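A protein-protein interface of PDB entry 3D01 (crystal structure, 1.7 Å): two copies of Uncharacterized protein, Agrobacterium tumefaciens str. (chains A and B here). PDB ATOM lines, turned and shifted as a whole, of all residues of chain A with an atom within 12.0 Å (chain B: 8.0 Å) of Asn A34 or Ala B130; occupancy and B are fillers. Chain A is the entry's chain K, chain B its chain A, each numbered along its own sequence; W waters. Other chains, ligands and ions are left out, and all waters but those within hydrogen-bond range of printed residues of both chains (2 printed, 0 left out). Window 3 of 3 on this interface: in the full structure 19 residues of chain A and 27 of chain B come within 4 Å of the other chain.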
ATOM      1  N   ASN A  34      26.892   5.192   9.639  1.00  0.00           N
ATOM      2  CA  ASN A  34      25.704   5.869  10.234  1.00  0.00           C
ATOM      3  C   ASN A  34      24.729   4.936  10.972  1.00  0.00           C
ATOM      4  O   ASN A  34      23.865   5.394  11.754  1.00  0.00           O
ATOM      5  CB  ASN A  34      24.998   6.710   9.173  1.00  0.00           C
ATOM      6  CG  ASN A  34      25.760   7.992   8.879  1.00  0.00           C
ATOM      7  OD1 ASN A  34      26.422   8.522   9.776  1.00  0.00           O
ATOM      8  ND2 ASN A  34      25.687   8.488   7.637  1.00  0.00           N
ATOM      9  N   TYR A  35      24.894   3.635  10.738  1.00  0.00           N
ATOM     10  CA  TYR A  35      24.346   2.613  11.627  1.00  0.00           C
ATOM     11  C   TYR A  35      25.503   1.843  12.248  1.00  0.00           C
ATOM     12  O   TYR A  35      26.605   1.787  11.692  1.00  0.00           O
ATOM     13  CB  TYR A  35      23.352   1.657  10.953  1.00  0.00           C
ATOM     14  CG  TYR A  35      23.909   0.900   9.803  1.00  0.00           C
ATOM     15  CD1 TYR A  35      24.246  -0.441   9.915  1.00  0.00           C
ATOM     16  CD2 TYR A  35      24.090   1.534   8.576  1.00  0.00           C
ATOM     17  CE1 TYR A  35      24.772  -1.139   8.819  1.00  0.00           C
ATOM     18  CE2 TYR A  35      24.623   0.874   7.503  1.00  0.00           C
ATOM     19  CZ  TYR A  35      24.956  -0.460   7.615  1.00  0.00           C
ATOM     20  OH  TYR A  35      25.477  -1.082   6.499  1.00  0.00           O
ATOM     21  N   VAL A  36      25.227   1.295  13.418  1.00  0.00           N
ATOM     22  CA  VAL A  36      26.202   0.650  14.246  1.00  0.00           C
ATOM     23  C   VAL A  36      25.816  -0.817  14.455  1.00  0.00           C
ATOM     24  O   VAL A  36      24.647  -1.159  14.331  1.00  0.00           O
ATOM     25  CB  VAL A  36      26.296   1.407  15.596  1.00  0.00           C
ATOM     26  CG1 VAL A  36      26.986   2.756  15.377  1.00  0.00           C
ATOM     27  CG2 VAL A  36      24.876   1.623  16.245  1.00  0.00           C
ATOM     28  N   PRO A  37      26.793  -1.677  14.818  1.00  0.00           N
ATOM     29  CA  PRO A  37      26.524  -3.106  15.089  1.00  0.00           C
ATOM     30  C   PRO A  37      25.632  -3.389  16.296  1.00  0.00           C
ATOM     31  O   PRO A  37      25.029  -4.465  16.385  1.00  0.00           O
ATOM     32  CB  PRO A  37      27.906  -3.715  15.314  1.00  0.00           C
ATOM     33  CG  PRO A  37      28.879  -2.598  15.310  1.00  0.00           C
ATOM     34  CD  PRO A  37      28.209  -1.325  14.963  1.00  0.00           C
ATOM     35  N   PHE A  38      25.589  -2.439  17.223  1.00  0.00           N
ATOM     36  CA  PHE A  38      24.759  -2.555  18.412  1.00  0.00           C
ATOM     37  C   PHE A  38      24.514  -1.227  19.097  1.00  0.00           C
ATOM     38  O   PHE A  38      25.270  -0.256  18.918  1.00  0.00           O
ATOM     39  CB  PHE A  38      25.373  -3.534  19.408  1.00  0.00           C
ATOM     40  CG  PHE A  38      26.739  -3.124  19.906  1.00  0.00           C
ATOM     41  CD1 PHE A  38      26.877  -2.210  20.945  1.00  0.00           C
ATOM     42  CD2 PHE A  38      27.875  -3.673  19.340  1.00  0.00           C
ATOM     43  CE1 PHE A  38      28.152  -1.836  21.392  1.00  0.00           C
ATOM     44  CE2 PHE A  38      29.141  -3.297  19.786  1.00  0.00           C
ATOM     45  CZ  PHE A  38      29.264  -2.374  20.818  1.00  0.00           C
ATOM     46  N   THR A  39      23.413  -1.191  19.841  1.00  0.00           N
ATOM     47  CA  THR A  39      23.090  -0.073  20.739  1.00  0.00           C
ATOM     48  C   THR A  39      22.655  -0.638  22.076  1.00  0.00           C
ATOM     49  O   THR A  39      22.234  -1.784  22.168  1.00  0.00           O
ATOM     50  CB  THR A  39      21.940   0.815  20.216  1.00  0.00           C
ATOM     51  OG1 THR A  39      20.782   0.017  19.943  1.00  0.00           O
ATOM     52  CG2 THR A  39      22.367   1.597  18.965  1.00  0.00           C
ATOM     53  N   TYR A  46      20.647  -4.183  21.809  1.00  0.00           N
ATOM     54  CA  TYR A  46      20.145  -4.413  20.453  1.00  0.00           C
ATOM     55  C   TYR A  46      21.289  -4.637  19.474  1.00  0.00           C
ATOM     56  O   TYR A  46      22.052  -3.743  19.238  1.00  0.00           O
ATOM     57  CB  TYR A  46      19.357  -3.199  19.972  1.00  0.00           C
ATOM     58  CG  TYR A  46      18.002  -3.185  20.528  1.00  0.00           C
ATOM     59  CD1 TYR A  46      16.922  -3.597  19.745  1.00  0.00           C
ATOM     60  CD2 TYR A  46      17.776  -2.794  21.834  1.00  0.00           C
ATOM     61  CE1 TYR A  46      15.655  -3.622  20.246  1.00  0.00           C
ATOM     62  CE2 TYR A  46      16.475  -2.805  22.360  1.00  0.00           C
ATOM     63  CZ  TYR A  46      15.436  -3.222  21.564  1.00  0.00           C
ATOM     64  OH  TYR A  46      14.147  -3.247  22.041  1.00  0.00           O
ATOM     65  N   SER A  48      22.493  -5.447  15.669  1.00  0.00           N
ATOM     66  CA  SER A  48      22.107  -5.364  14.234  1.00  0.00           C
ATOM     67  C   SER A  48      22.088  -6.747  13.556  1.00  0.00           C
ATOM     68  O   SER A  48      22.770  -7.694  14.005  1.00  0.00           O
ATOM     69  CB  SER A  48      23.100  -4.467  13.494  1.00  0.00           C
ATOM     70  OG  SER A  48      22.915  -3.142  13.889  1.00  0.00           O
ATOM     71  N   ARG B  17      17.839  21.017   9.703  1.00  0.00           N
ATOM     72  CA  ARG B  17      18.779  20.143   9.006  1.00  0.00           C
ATOM     73  C   ARG B  17      18.035  19.268   7.998  1.00  0.00           C
ATOM     74  O   ARG B  17      18.536  19.023   6.905  1.00  0.00           O
ATOM     75  CB  ARG B  17      19.533  19.252   9.983  1.00  0.00           C
ATOM     76  CG  ARG B  17      20.604  19.957  10.852  1.00  0.00           C
ATOM     77  CD  ARG B  17      20.961  19.064  12.011  1.00  0.00           C
ATOM     78  NE  ARG B  17      21.924  19.658  12.922  1.00  0.00           N
ATOM     79  CZ  ARG B  17      22.292  19.109  14.082  1.00  0.00           C
ATOM     80  NH1 ARG B  17      21.771  17.950  14.507  1.00  0.00           N
ATOM     81  NH2 ARG B  17      23.188  19.732  14.838  1.00  0.00           N
ATOM     82  N   LEU B  21      18.216  18.969   3.732  1.00  0.00           N
ATOM     83  CA  LEU B  21      18.230  17.751   2.894  1.00  0.00           C
ATOM     84  C   LEU B  21      17.078  17.712   1.882  1.00  0.00           C
ATOM     85  O   LEU B  21      17.045  16.841   1.001  1.00  0.00           O
ATOM     86  CB  LEU B  21      18.184  16.510   3.768  1.00  0.00           C
ATOM     87  CG  LEU B  21      19.371  16.277   4.682  1.00  0.00           C
ATOM     88  CD1 LEU B  21      19.128  15.075   5.589  1.00  0.00           C
ATOM     89  CD2 LEU B  21      20.622  16.083   3.855  1.00  0.00           C
ATOM     90  N   ALA B  81      11.905   7.357   6.629  1.00  0.00           N
ATOM     91  CA  ALA B  81      12.599   7.984   7.778  1.00  0.00           C
ATOM     92  C   ALA B  81      11.943   9.303   8.143  1.00  0.00           C
ATOM     93  O   ALA B  81      11.830   9.619   9.327  1.00  0.00           O
ATOM     94  CB  ALA B  81      14.104   8.157   7.501  1.00  0.00           C
ATOM     95  N   LEU B  85      10.212  10.223  11.694  1.00  0.00           N
ATOM     96  CA  LEU B  85      10.495  11.471  12.450  1.00  0.00           C
ATOM     97  C   LEU B  85       9.237  12.282  12.782  1.00  0.00           C
ATOM     98  O   LEU B  85       9.129  12.844  13.885  1.00  0.00           O
ATOM     99  CB  LEU B  85      11.509  12.330  11.710  1.00  0.00           C
ATOM    100  CG  LEU B  85      12.955  11.812  11.644  1.00  0.00           C
ATOM    101  CD1 LEU B  85      13.818  12.725  10.776  1.00  0.00           C
ATOM    102  CD2 LEU B  85      13.589  11.619  13.037  1.00  0.00           C
ATOM    103  N   ARG B 101      18.294   8.494  21.847  1.00  0.00           N
ATOM    104  CA  ARG B 101      19.012   7.603  20.928  1.00  0.00           C
ATOM    105  C   ARG B 101      18.001   6.854  20.052  1.00  0.00           C
ATOM    106  O   ARG B 101      16.992   6.374  20.550  1.00  0.00           O
ATOM    107  CB  ARG B 101      19.862   6.632  21.760  1.00  0.00           C
ATOM    108  CG  ARG B 101      20.304   5.351  21.118  1.00  0.00           C
ATOM    109  CD  ARG B 101      21.360   5.613  20.091  1.00  0.00           C
ATOM    110  NE  ARG B 101      22.548   6.092  20.762  1.00  0.00           N
ATOM    111  CZ  ARG B 101      23.653   6.518  20.159  1.00  0.00           C
ATOM    112  NH1 ARG B 101      24.684   6.929  20.902  1.00  0.00           N
ATOM    113  NH2 ARG B 101      23.733   6.547  18.836  1.00  0.00           N
ATOM    114  N   VAL B 102      18.278   6.794  18.750  1.00  0.00           N
ATOM    115  CA  VAL B 102      17.570   5.870  17.865  1.00  0.00           C
ATOM    116  C   VAL B 102      18.211   4.519  18.100  1.00  0.00           C
ATOM    117  O   VAL B 102      19.371   4.302  17.750  1.00  0.00           O
ATOM    118  CB  VAL B 102      17.684   6.267  16.375  1.00  0.00           C
ATOM    119  CG1 VAL B 102      16.910   5.281  15.478  1.00  0.00           C
ATOM    120  CG2 VAL B 102      17.227   7.725  16.182  1.00  0.00           C
ATOM    121  N   LEU B 105      16.371   0.525  13.761  1.00  0.00           N
ATOM    122  CA  LEU B 105      15.493   0.611  12.595  1.00  0.00           C
ATOM    123  C   LEU B 105      15.416  -0.767  11.973  1.00  0.00           C
ATOM    124  O   LEU B 105      16.440  -1.426  11.822  1.00  0.00           O
ATOM    125  CB  LEU B 105      16.011   1.602  11.536  1.00  0.00           C
ATOM    126  CG  LEU B 105      16.131   3.082  11.902  1.00  0.00           C
ATOM    127  CD1 LEU B 105      16.558   3.823  10.646  1.00  0.00           C
ATOM    128  CD2 LEU B 105      14.873   3.664  12.491  1.00  0.00           C
ATOM    129  N   ASN B 123      20.406   2.459   3.703  1.00  0.00           N
ATOM    130  CA  ASN B 123      21.359   3.578   3.912  1.00  0.00           C
ATOM    131  C   ASN B 123      20.677   4.920   3.656  1.00  0.00           C
ATOM    132  O   ASN B 123      21.006   5.901   4.317  1.00  0.00           O
ATOM    133  CB  ASN B 123      22.652   3.464   3.072  1.00  0.00           C
ATOM    134  CG  ASN B 123      23.612   2.348   3.536  1.00  0.00           C
ATOM    135  OD1 ASN B 123      24.521   1.994   2.809  1.00  0.00           O
ATOM    136  ND2 ASN B 123      23.433   1.832   4.735  1.00  0.00           N
ATOM    137  N   GLY B 124      19.704   4.985   2.740  1.00  0.00           N
ATOM    138  CA  GLY B 124      18.886   6.190   2.528  1.00  0.00           C
ATOM    139  C   GLY B 124      18.319   6.757   3.830  1.00  0.00           C
ATOM    140  O   GLY B 124      18.504   7.946   4.165  1.00  0.00           O
ATOM    141  N   ALA B 125      17.690   5.872   4.603  1.00  0.00           N
ATOM    142  CA  ALA B 125      17.107   6.228   5.892  1.00  0.00           C
ATOM    143  C   ALA B 125      18.225   6.459   6.927  1.00  0.00           C
ATOM    144  O   ALA B 125      18.222   7.453   7.661  1.00  0.00           O
ATOM    145  CB  ALA B 125      16.153   5.104   6.361  1.00  0.00           C
ATOM    146  N   SER B 126      19.167   5.537   7.022  1.00  0.00           N
ATOM    147  CA  SER B 126      20.199   5.627   8.069  1.00  0.00           C
ATOM    148  C   SER B 126      21.006   6.929   7.965  1.00  0.00           C
ATOM    149  O   SER B 126      21.315   7.569   8.984  1.00  0.00           O
ATOM    150  CB  SER B 126      21.134   4.418   8.028  1.00  0.00           C
ATOM    151  OG  SER B 126      20.459   3.222   8.388  1.00  0.00           O
ATOM    152  N   ASN B 127      21.371   7.302   6.742  1.00  0.00           N
ATOM    153  CA  ASN B 127      22.163   8.523   6.507  1.00  0.00           C
ATOM    154  C   ASN B 127      21.386   9.786   6.866  1.00  0.00           C
ATOM    155  O   ASN B 127      21.917  10.687   7.535  1.00  0.00           O
ATOM    156  CB  ASN B 127      22.635   8.580   5.067  1.00  0.00           C
ATOM    157  CG  ASN B 127      23.668   7.501   4.732  1.00  0.00           C
ATOM    158  OD1 ASN B 127      24.257   6.890   5.609  1.00  0.00           O
ATOM    159  ND2 ASN B 127      23.886   7.275   3.453  1.00  0.00           N
ATOM    160  N   LEU B 128      20.116   9.829   6.485  1.00  0.00           N
ATOM    161  CA  LEU B 128      19.231  10.960   6.814  1.00  0.00           C
ATOM    162  C   LEU B 128      19.059  11.119   8.320  1.00  0.00           C
ATOM    163  O   LEU B 128      19.200  12.217   8.858  1.00  0.00           O
ATOM    164  CB  LEU B 128      17.858  10.782   6.161  1.00  0.00           C
ATOM    165  CG  LEU B 128      16.807  11.879   6.363  1.00  0.00           C
ATOM    166  CD1 LEU B 128      15.842  11.972   5.168  1.00  0.00           C
ATOM    167  CD2 LEU B 128      16.050  11.703   7.675  1.00  0.00           C
ATOM    168  N   ILE B 129      18.720  10.029   8.993  1.00  0.00           N
ATOM    169  CA  ILE B 129      18.545  10.026  10.445  1.00  0.00           C
ATOM    170  C   ILE B 129      19.810  10.503  11.182  1.00  0.00           C
ATOM    171  O   ILE B 129      19.733  11.375  12.056  1.00  0.00           O
ATOM    172  CB  ILE B 129      18.107   8.604  10.950  1.00  0.00           C
ATOM    173  CG1 ILE B 129      16.678   8.255  10.483  1.00  0.00           C
ATOM    174  CG2 ILE B 129      18.255   8.470  12.476  1.00  0.00           C
ATOM    175  CD1 ILE B 129      15.585   9.230  10.902  1.00  0.00           C
ATOM    176  N   ALA B 130      20.958   9.929  10.824  1.00  0.00           N
ATOM    177  CA  ALA B 130      22.233  10.283  11.423  1.00  0.00           C
ATOM    178  C   ALA B 130      22.603  11.742  11.138  1.00  0.00           C
ATOM    179  O   ALA B 130      23.120  12.416  12.022  1.00  0.00           O
ATOM    180  CB  ALA B 130      23.313   9.366  10.912  1.00  0.00           C
ATOM    181  N   THR B 131      22.329  12.215   9.922  1.00  0.00           N
ATOM    182  CA  THR B 131      22.567  13.612   9.543  1.00  0.00           C
ATOM    183  C   THR B 131      21.756  14.620  10.374  1.00  0.00           C
ATOM    184  O   THR B 131      22.308  15.585  10.887  1.00  0.00           O
ATOM    185  CB  THR B 131      22.306  13.826   8.045  1.00  0.00           C
ATOM    186  OG1 THR B 131      23.248  13.042   7.298  1.00  0.00           O
ATOM    187  CG2 THR B 131      22.442  15.310   7.637  1.00  0.00           C
ATOM    188  N   VAL B 132      20.462  14.405  10.539  1.00  0.00           N
ATOM    189  CA  VAL B 132      19.638  15.422  11.179  1.00  0.00           C
ATOM    190  C   VAL B 132      19.729  15.329  12.700  1.00  0.00           C
ATOM    191  O   VAL B 132      19.557  16.333  13.385  1.00  0.00           O
ATOM    192  CB  VAL B 132      18.170  15.393  10.680  1.00  0.00           C
ATOM    193  CG1 VAL B 132      18.126  15.377   9.153  1.00  0.00           C
ATOM    194  CG2 VAL B 132      17.372  14.209  11.296  1.00  0.00           C
ATOM    195  N   LEU B 133      20.076  14.149  13.227  1.00  0.00           N
ATOM    196  CA  LEU B 133      20.160  13.949  14.679  1.00  0.00           C
ATOM    197  C   LEU B 133      21.580  13.944  15.211  1.00  0.00           C
ATOM    198  O   LEU B 133      21.773  14.107  16.421  1.00  0.00           O
ATOM    199  CB  LEU B 133      19.467  12.637  15.110  1.00  0.00           C
ATOM    200  CG  LEU B 133      17.950  12.525  14.931  1.00  0.00           C
ATOM    201  CD1 LEU B 133      17.454  11.138  15.424  1.00  0.00           C
ATOM    202  CD2 LEU B 133      17.210  13.693  15.663  1.00  0.00           C
ATOM    203  N   GLY B 134      22.569  13.754  14.346  1.00  0.00           N
ATOM    204  CA  GLY B 134      23.944  13.544  14.795  1.00  0.00           C
ATOM    205  C   GLY B 134      24.150  12.222  15.535  1.00  0.00           C
ATOM    206  O   GLY B 134      23.535  11.199  15.196  1.00  0.00           O
ATOM    207  N   GLU B 135      24.981  12.241  16.576  1.00  0.00           N
ATOM    208  CA  GLU B 135      25.433  11.006  17.186  1.00  0.00           C
ATOM    209  C   GLU B 135      24.277  10.183  17.733  1.00  0.00           C
ATOM    210  O   GLU B 135      24.281   8.964  17.569  1.00  0.00           O
ATOM    211  CB  GLU B 135      26.517  11.255  18.259  1.00  0.00           C
ATOM    212  CG  GLU B 135      26.959  10.025  19.077  1.00  0.00           C
ATOM    213  CD  GLU B 135      27.514   8.875  18.237  1.00  0.00           C
ATOM    214  OE1 GLU B 135      28.239   9.128  17.235  1.00  0.00           O
ATOM    215  OE2 GLU B 135      27.225   7.702  18.601  1.00  0.00           O
ATOM    216  N   PRO B 136      23.297  10.820  18.387  1.00  0.00           N
ATOM    217  CA  PRO B 136      22.107  10.088  18.869  1.00  0.00           C
ATOM    218  C   PRO B 136      21.284   9.409  17.766  1.00  0.00           C
ATOM    219  O   PRO B 136      20.462   8.570  18.065  1.00  0.00           O
ATOM    220  CB  PRO B 136      21.243  11.178  19.477  1.00  0.00           C
ATOM    221  CG  PRO B 136      22.222  12.257  19.874  1.00  0.00           C
ATOM    222  CD  PRO B 136      23.243  12.244  18.775  1.00  0.00           C
ATOM    223  N   GLY B 137      21.450   9.851  16.527  1.00  0.00           N
ATOM    224  CA  GLY B 137      20.824   9.200  15.388  1.00  0.00           C
ATOM    225  C   GLY B 137      21.433   7.906  14.899  1.00  0.00           C
ATOM    226  O   GLY B 137      20.793   7.209  14.067  1.00  0.00           O
ATOM    227  N   ARG B 138      22.639   7.574  15.362  1.00  0.00           N
ATOM    228  CA  ARG B 138      23.304   6.320  14.950  1.00  0.00           C
ATOM    229  C   ARG B 138      22.647   5.117  15.662  1.00  0.00           C
ATOM    230  O   ARG B 138      22.528   5.101  16.883  1.00  0.00           O
ATOM    231  CB  ARG B 138      24.802   6.389  15.213  1.00  0.00           C
ATOM    232  CG  ARG B 138      25.504   7.294  14.215  1.00  0.00           C
ATOM    233  CD  ARG B 138      26.878   7.699  14.664  1.00  0.00           C
ATOM    234  NE  ARG B 138      27.847   6.619  14.902  1.00  0.00           N
ATOM    235  CZ  ARG B 138      28.435   5.877  13.957  1.00  0.00           C
ATOM    236  NH1 ARG B 138      28.120   6.017  12.665  1.00  0.00           N
ATOM    237  NH2 ARG B 138      29.343   4.964  14.307  1.00  0.00           N
ATOM    238  N   HIS B 139      22.227   4.113  14.894  1.00  0.00           N
ATOM    239  CA  HIS B 139      21.305   3.092  15.375  1.00  0.00           C
ATOM    240  C   HIS B 139      21.755   1.702  14.959  1.00  0.00           C
ATOM    241  O   HIS B 139      22.518   1.559  13.998  1.00  0.00           O
ATOM    242  CB  HIS B 139      19.932   3.361  14.745  1.00  0.00           C
ATOM    243  CG  HIS B 139      20.024   3.680  13.289  1.00  0.00           C
ATOM    244  ND1 HIS B 139      20.318   4.950  12.829  1.00  0.00           N
ATOM    245  CD2 HIS B 139      19.940   2.888  12.190  1.00  0.00           C
ATOM    246  CE1 HIS B 139      20.397   4.926  11.510  1.00  0.00           C
ATOM    247  NE2 HIS B 139      20.167   3.690  11.098  1.00  0.00           N
ATOM    248  N   ALA B 140      21.296   0.695  15.696  1.00  0.00           N
ATOM    249  CA  ALA B 140      21.332  -0.695  15.237  1.00  0.00           C
ATOM    250  C   ALA B 140      20.300  -0.837  14.112  1.00  0.00           C
ATOM    251  O   ALA B 140      19.412  -0.024  13.988  1.00  0.00           O
ATOM    252  CB  ALA B 140      21.005  -1.645  16.342  1.00  0.00           C
ATOM    253  N   ARG B 141      20.415  -1.898  13.318  1.00  0.00           N
ATOM    254  CA  ARG B 141      19.629  -2.020  12.099  1.00  0.00           C
ATOM    255  C   ARG B 141      19.498  -3.456  11.600  1.00  0.00           C
ATOM    256  O   ARG B 141      20.405  -4.266  11.785  1.00  0.00           O
ATOM    257  CB  ARG B 141      20.324  -1.249  10.985  1.00  0.00           C
ATOM    258  CG  ARG B 141      19.403  -0.777   9.971  1.00  0.00           C
ATOM    259  CD  ARG B 141      20.123   0.070   8.923  1.00  0.00           C
ATOM    260  NE  ARG B 141      20.946  -0.704   7.979  1.00  0.00           N
ATOM    261  CZ  ARG B 141      21.559  -0.156   6.914  1.00  0.00           C
ATOM    262  NH1 ARG B 141      21.458   1.122   6.701  1.00  0.00           N
ATOM    263  NH2 ARG B 141      22.276  -0.881   6.066  1.00  0.00           N
HETATM  264  O   HOH W   1      25.798   4.503   6.709  1.00  0.00           O
HETATM  265  O   HOH W   2      26.154   0.114   4.211  1.00  0.00           O
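OE1 of Glu B135 is in salt-bridge range of NE of Arg B138 (3.4 Å). O of Asn B127 is in hydrogen-bond range of OG1 of Thr B131, at 2.7 Å. The guanidinium group (NH2) of Arg B101 sits at hydrogen-bond distance from the backbone carbonyl oxygen (O) of Arg B138 (2.7 Å). The backbone carbonyl oxygen (O) of Asn B123 sits close to the side-chain amide nitrogen (ND2) of Asn B127, at 3.3 Å. The side-chain amide nitrogen of Asn B123 lies close to the guanidinium group of Arg B141. The backbone carbonyl oxygen (O) of Gly B137 sits at hydrogen-bond distance from a ring nitrogen (ND1) of His B139, at 2.6 Å.
Of the 8 printed residues of chain A, 6 touch a printed residue of chain B. Hydrophobic or aromatic side chains of chain A within 4 Å of the printed part of chain B: Tyr A35 and Val A36. Of the 26 printed residues of chain B, 8 touch a printed residue of chain A. Hydrophobic or aromatic side chains of chain B within 4 Å of the printed part of chain A: Ala B130, His B139 and Ala B140. Among the printed residues, 15 pairs touch across the chains.
Of the printed residues of chain B, Asn A34 touches Ser B126 (3.8 Å), Asn B127 (3.0 Å), Ala B130 (3.4 Å), Arg B138 (3.4 Å) and His B139 (3.5 Å). Of the printed residues of chain B, Val A36 touches Arg B138 (3.4 Å), His B139 (2.8 Å) and Ala B140 (3.5 Å). Of the printed residues of chain B, Ser A48 touches Ala B140 and Arg B141. Arg B17 touches none of the printed residues of chain A. Of the printed residues of chain A, Asn B123 touches Tyr A35 (3.2 Å). Gly B124 touches none of the printed residues of chain A. Of the printed residues of chain A, Ser B126 touches Asn A34 (3.8 Å). Of chain A, only Asn A34 comes within 4 Å of Asn B127. No residue of chain A comes within 4 Å of Leu B128. Ile B129 touches none of the printed residues of chain A. Ala B130 touches one residue of chain A. No residue of chain A comes within 4 Å of Thr B131. No residue of chain A comes within 4 Å of Val B132. No residue of chain A comes within 4 Å of Leu B133. No residue of chain A comes within 4 Å of Pro B136. His B139 touches just these residues of chain A: Asn A34 (3.5 Å), Tyr A35 (3.2 Å) and Val A36 (2.8 Å). Printed residues of chain A within 4 Å of Ala B140: Val A36 (3.5 Å), Thr A39 (3.6 Å), Tyr A46 (3.7 Å) and Ser A48 (3.2 Å). The nearest residue of chain A that does not touch Ala B130 is Tyr A35 (5.9 Å). The nearest printed residue of chain A that does not touch Arg B141 is Val A36 (4.4 Å).
Ser B126 touches Asn A34 (O to CB, 3.8 Å). Asn A34 touches Ala B130. His B139 touches Asn A34 (CE1 to O, 3.5 Å). Tyr A35 touches Asn B123. O of His B139 touches CB of Tyr A35, 3.2 Å away. Arg B138 touches Val A36. Val A36 touches Ala B140. N of Ala B140 touches CG2 of Thr A39, 3.6 Å away. O of Tyr A46 touches CB of Ala B140, at 3.7 Å. Ser A48 touches Ala B140 (OG to CA, 3.2 Å).
Water W2 lies within hydrogen-bond range of the side-chain hydroxyl (OH) of Tyr A35 (2.7 Å) and the side-chain amide oxygen (OD1) of Asn B123 (2.9 Å). Water W1 lies within hydrogen-bond range of the side-chain amide oxygen of Asn B127 (3.0 Å) and the backbone NH of Asn A34 (3.2 Å).
The side-chain amide nitrogen (ND2) of Asn A34 sits at hydrogen-bond distance from the side-chain amide oxygen (OD1) of Asn B127, at 3.0 Å. The backbone NH (N) of Val A36 is in hydrogen-bond range of the backbone carbonyl oxygen (O) of His B139 (2.8 Å). OH of Tyr A35 sits close to NH2 of Arg B141. The backbone NH (N) of Arg B141 is in hydrogen-bond range of the side-chain hydroxyl (OG) of Ser A48 (2.9 Å). N of Asn A34 sits close to NH1 of Arg B138 (3.4 Å).
No position is printed for both chains.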
